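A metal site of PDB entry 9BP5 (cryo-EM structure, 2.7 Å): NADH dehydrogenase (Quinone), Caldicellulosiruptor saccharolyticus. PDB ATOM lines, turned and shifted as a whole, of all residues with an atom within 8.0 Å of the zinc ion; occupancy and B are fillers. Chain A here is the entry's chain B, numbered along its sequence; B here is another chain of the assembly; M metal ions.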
ATOM      1  N   GLY A   6       6.587 -24.685  21.437  1.00  0.00           N
ATOM      2  CA  GLY A   6       7.862 -24.954  22.074  1.00  0.00           C
ATOM      3  C   GLY A   6       8.098 -26.429  22.286  1.00  0.00           C
ATOM      4  O   GLY A   6       7.646 -27.015  23.267  1.00  0.00           O
ATOM      5  N   LEU A   7       8.811 -27.047  21.343  1.00  0.00           N
ATOM      6  CA  LEU A   7       9.102 -28.475  21.371  1.00  0.00           C
ATOM      7  C   LEU A   7      10.545 -28.699  21.823  1.00  0.00           C
ATOM      8  O   LEU A   7      11.440 -28.975  21.034  1.00  0.00           O
ATOM      9  CB  LEU A   7       8.845 -29.093  20.005  1.00  0.00           C
ATOM     10  CG  LEU A   7       7.399 -29.030  19.524  1.00  0.00           C
ATOM     11  CD1 LEU A   7       7.295 -29.691  18.184  1.00  0.00           C
ATOM     12  CD2 LEU A   7       6.489 -29.700  20.530  1.00  0.00           C
ATOM     13  N   GLY A   8      10.758 -28.567  23.122  1.00  0.00           N
ATOM     14  CA  GLY A   8      11.986 -29.009  23.748  1.00  0.00           C
ATOM     15  C   GLY A   8      11.860 -30.428  24.230  1.00  0.00           C
ATOM     16  O   GLY A   8      10.910 -31.150  23.910  1.00  0.00           O
ATOM     17  N   SER A   9      12.852 -30.850  25.014  1.00  0.00           N
ATOM     18  CA  SER A   9      12.714 -32.127  25.719  1.00  0.00           C
ATOM     19  C   SER A   9      11.550 -32.066  26.690  1.00  0.00           C
ATOM     20  O   SER A   9      10.789 -33.039  26.830  1.00  0.00           O
ATOM     21  CB  SER A   9      14.011 -32.467  26.447  1.00  0.00           C
ATOM     22  OG  SER A   9      13.754 -33.219  27.625  1.00  0.00           O
ATOM     23  N   CYS A  10      11.382 -30.940  27.387  1.00  0.00           N
ATOM     24  CA  CYS A  10      10.226 -30.719  28.233  1.00  0.00           C
ATOM     25  C   CYS A  10       8.990 -30.306  27.446  1.00  0.00           C
ATOM     26  O   CYS A  10       7.872 -30.455  27.963  1.00  0.00           O
ATOM     27  CB  CYS A  10      10.541 -29.645  29.277  1.00  0.00           C
ATOM     28  SG  CYS A  10      11.612 -28.329  28.669  1.00  0.00           S
ATOM     29  N   GLY A  11       9.157 -29.782  26.234  1.00  0.00           N
ATOM     30  CA  GLY A  11       8.002 -29.376  25.444  1.00  0.00           C
ATOM     31  C   GLY A  11       7.113 -30.542  25.069  1.00  0.00           C
ATOM     32  O   GLY A  11       5.895 -30.490  25.231  1.00  0.00           O
ATOM     33  N   MET A  12       7.714 -31.624  24.555  1.00  0.00           N
ATOM     34  CA  MET A  12       6.942 -32.817  24.253  1.00  0.00           C
ATOM     35  C   MET A  12       6.618 -33.648  25.490  1.00  0.00           C
ATOM     36  O   MET A  12       5.831 -34.588  25.397  1.00  0.00           O
ATOM     37  CB  MET A  12       7.658 -33.688  23.226  1.00  0.00           C
ATOM     38  CG  MET A  12       8.386 -32.907  22.161  1.00  0.00           C
ATOM     39  SD  MET A  12       8.504 -33.895  20.667  1.00  0.00           S
ATOM     40  CE  MET A  12      10.064 -33.364  19.999  1.00  0.00           C
ATOM     41  N   ALA A  14       5.192 -32.139  28.045  1.00  0.00           N
ATOM     42  CA  ALA A  14       4.029 -31.459  28.570  1.00  0.00           C
ATOM     43  C   ALA A  14       2.878 -31.410  27.573  1.00  0.00           C
ATOM     44  O   ALA A  14       1.925 -30.652  27.776  1.00  0.00           O
ATOM     45  CB  ALA A  14       4.402 -30.038  29.013  1.00  0.00           C
ATOM     46  N   GLY A  40      12.656 -24.252  20.561  1.00  0.00           N
ATOM     47  CA  GLY A  40      13.242 -24.802  21.755  1.00  0.00           C
ATOM     48  C   GLY A  40      12.577 -24.305  23.017  1.00  0.00           C
ATOM     49  O   GLY A  40      11.445 -23.827  23.017  1.00  0.00           O
ATOM     50  N   CYS A  41      13.315 -24.405  24.122  1.00  0.00           N
ATOM     51  CA  CYS A  41      12.832 -23.978  25.425  1.00  0.00           C
ATOM     52  C   CYS A  41      13.301 -22.556  25.700  1.00  0.00           C
ATOM     53  O   CYS A  41      14.513 -22.294  25.727  1.00  0.00           O
ATOM     54  CB  CYS A  41      13.314 -24.924  26.517  1.00  0.00           C
ATOM     55  SG  CYS A  41      12.622 -24.616  28.160  1.00  0.00           S
ATOM     56  N   ILE A  42      12.355 -21.634  25.896  1.00  0.00           N
ATOM     57  CA  ILE A  42      12.699 -20.249  26.183  1.00  0.00           C
ATOM     58  C   ILE A  42      13.187 -20.065  27.614  1.00  0.00           C
ATOM     59  O   ILE A  42      13.737 -19.008  27.943  1.00  0.00           O
ATOM     60  CB  ILE A  42      11.499 -19.328  25.908  1.00  0.00           C
ATOM     61  CG1 ILE A  42      11.941 -17.870  25.768  1.00  0.00           C
ATOM     62  CG2 ILE A  42      10.486 -19.445  27.022  1.00  0.00           C
ATOM     63  CD1 ILE A  42      10.800 -16.892  25.729  1.00  0.00           C
ATOM     64  N   GLY A  43      13.025 -21.075  28.458  1.00  0.00           N
ATOM     65  CA  GLY A  43      13.391 -21.005  29.850  1.00  0.00           C
ATOM     66  C   GLY A  43      12.213 -21.024  30.800  1.00  0.00           C
ATOM     67  O   GLY A  43      12.383 -21.363  31.976  1.00  0.00           O
ATOM     68  N   LEU A  44      11.019 -20.687  30.321  1.00  0.00           N
ATOM     69  CA  LEU A  44       9.797 -20.757  31.124  1.00  0.00           C
ATOM     70  C   LEU A  44       9.239 -22.179  31.032  1.00  0.00           C
ATOM     71  O   LEU A  44       8.147 -22.415  30.514  1.00  0.00           O
ATOM     72  CB  LEU A  44       8.791 -19.723  30.662  1.00  0.00           C
ATOM     73  CG  LEU A  44       9.322 -18.314  30.384  1.00  0.00           C
ATOM     74  CD1 LEU A  44       8.370 -17.564  29.455  1.00  0.00           C
ATOM     75  CD2 LEU A  44       9.518 -17.557  31.670  1.00  0.00           C
ATOM     76  N   CYS A  45      10.015 -23.125  31.554  1.00  0.00           N
ATOM     77  CA  CYS A  45       9.628 -24.532  31.496  1.00  0.00           C
ATOM     78  C   CYS A  45       8.421 -24.846  32.364  1.00  0.00           C
ATOM     79  O   CYS A  45       7.868 -25.947  32.257  1.00  0.00           O
ATOM     80  CB  CYS A  45      10.805 -25.420  31.889  1.00  0.00           C
ATOM     81  SG  CYS A  45      12.216 -25.327  30.763  1.00  0.00           S
ATOM     82  N   PHE A  46       8.009 -23.931  33.228  1.00  0.00           N
ATOM     83  CA  PHE A  46       6.813 -24.095  34.050  1.00  0.00           C
ATOM     84  C   PHE A  46       5.567 -23.542  33.366  1.00  0.00           C
ATOM     85  O   PHE A  46       4.506 -23.509  33.993  1.00  0.00           O
ATOM     86  CB  PHE A  46       7.007 -23.423  35.408  1.00  0.00           C
ATOM     87  CG  PHE A  46       7.218 -21.944  35.331  1.00  0.00           C
ATOM     88  CD1 PHE A  46       8.436 -21.416  34.932  1.00  0.00           C
ATOM     89  CD2 PHE A  46       6.210 -21.067  35.683  1.00  0.00           C
ATOM     90  CE1 PHE A  46       8.635 -20.060  34.865  1.00  0.00           C
ATOM     91  CE2 PHE A  46       6.397 -19.713  35.623  1.00  0.00           C
ATOM     92  CZ  PHE A  46       7.611 -19.212  35.210  1.00  0.00           C
ATOM     93  N   PHE A  47       5.679 -23.089  32.120  1.00  0.00           N
ATOM     94  CA  PHE A  47       4.543 -22.609  31.344  1.00  0.00           C
ATOM     95  C   PHE A  47       4.324 -23.408  30.075  1.00  0.00           C
ATOM     96  O   PHE A  47       3.505 -23.019  29.239  1.00  0.00           O
ATOM     97  CB  PHE A  47       4.733 -21.126  30.989  1.00  0.00           C
ATOM     98  CG  PHE A  47       4.126 -20.192  31.997  1.00  0.00           C
ATOM     99  CD1 PHE A  47       2.810 -20.344  32.388  1.00  0.00           C
ATOM    100  CD2 PHE A  47       4.871 -19.167  32.539  1.00  0.00           C
ATOM    101  CE1 PHE A  47       2.252 -19.486  33.310  1.00  0.00           C
ATOM    102  CE2 PHE A  47       4.325 -18.310  33.467  1.00  0.00           C
ATOM    103  CZ  PHE A  47       3.014 -18.466  33.850  1.00  0.00           C
ATOM    104  N   GLU A  48       5.035 -24.531  29.903  1.00  0.00           N
ATOM    105  CA  GLU A  48       4.868 -25.338  28.713  1.00  0.00           C
ATOM    106  C   GLU A  48       3.486 -26.004  28.699  1.00  0.00           C
ATOM    107  O   GLU A  48       2.956 -26.366  29.748  1.00  0.00           O
ATOM    108  CB  GLU A  48       5.956 -26.398  28.626  1.00  0.00           C
ATOM    109  CG  GLU A  48       7.330 -25.895  29.020  1.00  0.00           C
ATOM    110  CD  GLU A  48       8.213 -25.629  27.822  1.00  0.00           C
ATOM    111  OE1 GLU A  48       7.690 -25.610  26.695  1.00  0.00           O
ATOM    112  OE2 GLU A  48       9.429 -25.436  28.013  1.00  0.00           O
ATOM    113  N   LEU A  50       4.220 -23.759  25.198  1.00  0.00           N
ATOM    114  CA  LEU A  50       4.200 -22.339  24.868  1.00  0.00           C
ATOM    115  C   LEU A  50       3.942 -22.169  23.381  1.00  0.00           C
ATOM    116  O   LEU A  50       4.609 -22.793  22.561  1.00  0.00           O
ATOM    117  CB  LEU A  50       5.515 -21.670  25.257  1.00  0.00           C
ATOM    118  CG  LEU A  50       5.815 -21.522  26.751  1.00  0.00           C
ATOM    119  CD1 LEU A  50       7.273 -21.150  26.955  1.00  0.00           C
ATOM    120  CD2 LEU A  50       4.912 -20.486  27.367  1.00  0.00           C
ATOM    121  N   PHE A 190      20.037 -29.952  32.660  1.00  0.00           N
ATOM    122  CA  PHE A 190      19.466 -30.100  31.326  1.00  0.00           C
ATOM    123  C   PHE A 190      19.789 -28.917  30.420  1.00  0.00           C
ATOM    124  O   PHE A 190      19.086 -28.706  29.418  1.00  0.00           O
ATOM    125  CB  PHE A 190      17.955 -30.277  31.408  1.00  0.00           C
ATOM    126  CG  PHE A 190      17.271 -29.340  32.351  1.00  0.00           C
ATOM    127  CD1 PHE A 190      17.099 -29.669  33.682  1.00  0.00           C
ATOM    128  CD2 PHE A 190      16.794 -28.122  31.905  1.00  0.00           C
ATOM    129  CE1 PHE A 190      16.472 -28.802  34.540  1.00  0.00           C
ATOM    130  CE2 PHE A 190      16.163 -27.252  32.771  1.00  0.00           C
ATOM    131  CZ  PHE A 190      16.004 -27.595  34.091  1.00  0.00           C
ATOM    132  N   SER A 194      18.903 -28.703  26.280  1.00  0.00           N
ATOM    133  CA  SER A 194      18.041 -27.646  25.774  1.00  0.00           C
ATOM    134  C   SER A 194      18.749 -26.780  24.746  1.00  0.00           C
ATOM    135  O   SER A 194      18.139 -26.327  23.775  1.00  0.00           O
ATOM    136  CB  SER A 194      17.532 -26.786  26.938  1.00  0.00           C
ATOM    137  OG  SER A 194      16.651 -27.532  27.763  1.00  0.00           O
ATOM    138  N   GLU A 197      18.749 -28.746  21.582  1.00  0.00           N
ATOM    139  CA  GLU A 197      17.411 -28.808  21.030  1.00  0.00           C
ATOM    140  C   GLU A 197      16.886 -27.464  20.553  1.00  0.00           C
ATOM    141  O   GLU A 197      15.890 -27.429  19.824  1.00  0.00           O
ATOM    142  CB  GLU A 197      16.439 -29.370  22.066  1.00  0.00           C
ATOM    143  CG  GLU A 197      16.597 -30.851  22.313  1.00  0.00           C
ATOM    144  CD  GLU A 197      16.114 -31.260  23.673  1.00  0.00           C
ATOM    145  OE1 GLU A 197      15.426 -30.441  24.326  1.00  0.00           O
ATOM    146  OE2 GLU A 197      16.396 -32.394  24.089  1.00  0.00           O
ATOM    147  N   GLY A 350      10.978 -22.756  37.995  1.00  0.00           N
ATOM    148  CA  GLY A 350      12.177 -23.470  37.600  1.00  0.00           C
ATOM    149  C   GLY A 350      12.364 -23.526  36.105  1.00  0.00           C
ATOM    150  O   GLY A 350      11.416 -23.290  35.350  1.00  0.00           O
ATOM    151  N   GLY A 351      13.570 -23.823  35.655  1.00  0.00           N
ATOM    152  CA  GLY A 351      13.856 -23.915  34.239  1.00  0.00           C
ATOM    153  C   GLY A 351      15.235 -23.380  33.945  1.00  0.00           C
ATOM    154  O   GLY A 351      16.066 -23.235  34.825  1.00  0.00           O
ATOM    155  N   LEU A 352      15.472 -23.085  32.664  1.00  0.00           N
ATOM    156  CA  LEU A 352      16.759 -22.561  32.242  1.00  0.00           C
ATOM    157  C   LEU A 352      16.826 -21.067  32.506  1.00  0.00           C
ATOM    158  O   LEU A 352      15.915 -20.319  32.119  1.00  0.00           O
ATOM    159  CB  LEU A 352      16.995 -22.840  30.759  1.00  0.00           C
ATOM    160  CG  LEU A 352      17.740 -24.118  30.369  1.00  0.00           C
ATOM    161  CD1 LEU A 352      18.279 -23.978  28.973  1.00  0.00           C
ATOM    162  CD2 LEU A 352      18.847 -24.410  31.350  1.00  0.00           C
ATOM    163  N   GLY B 139      14.508 -34.297  31.403  1.00  0.00           N
ATOM    164  CA  GLY B 139      14.372 -32.980  30.839  1.00  0.00           C
ATOM    165  C   GLY B 139      13.212 -32.177  31.398  1.00  0.00           C
ATOM    166  O   GLY B 139      13.312 -30.953  31.492  1.00  0.00           O
ATOM    167  N   CYS B 140      12.127 -32.846  31.781  1.00  0.00           N
ATOM    168  CA  CYS B 140      10.936 -32.176  32.295  1.00  0.00           C
ATOM    169  C   CYS B 140      10.995 -32.173  33.822  1.00  0.00           C
ATOM    170  O   CYS B 140      10.304 -32.913  34.502  1.00  0.00           O
ATOM    171  CB  CYS B 140       9.681 -32.879  31.796  1.00  0.00           C
ATOM    172  SG  CYS B 140       9.792 -34.673  31.803  1.00  0.00           S
ATOM    173  N   CYS B 141      11.851 -31.296  34.353  1.00  0.00           N
ATOM    174  CA  CYS B 141      11.998 -31.203  35.801  1.00  0.00           C
ATOM    175  C   CYS B 141      10.778 -30.564  36.447  1.00  0.00           C
ATOM    176  O   CYS B 141      10.465 -30.874  37.599  1.00  0.00           O
ATOM    177  CB  CYS B 141      13.252 -30.405  36.151  1.00  0.00           C
ATOM    178  SG  CYS B 141      14.742 -31.387  36.337  1.00  0.00           S
ATOM    179  N   SER B 142      10.080 -29.688  35.730  1.00  0.00           N
ATOM    180  CA  SER B 142       8.951 -28.970  36.317  1.00  0.00           C
ATOM    181  C   SER B 142       7.757 -29.868  36.585  1.00  0.00           C
ATOM    182  O   SER B 142       6.845 -29.448  37.304  1.00  0.00           O
ATOM    183  CB  SER B 142       8.528 -27.815  35.407  1.00  0.00           C
ATOM    184  OG  SER B 142       8.010 -26.745  36.174  1.00  0.00           O
HETATM  185 ZN    ZN M   1      11.061 -26.119  28.942  1.00  0.00          ZN
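SG of Cys 41 lies close to N of Gly 43.
Within 4 Å of the zinc ion: Cys 10, Cys 41, Cys 45 and Glu 48.
The nearest printed residue that does not touch the zinc ion is Leu 44 (4.8 Å).
OE2 of Glu 48 binds the zinc ion, at 2.0 Å.
The zinc ion is bound by SG of Cys 10 (2.3 Å).
SG of Cys 45 is bound to the zinc ion.
The zinc ion is bound by SG of Cys 41, at 2.3 Å.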
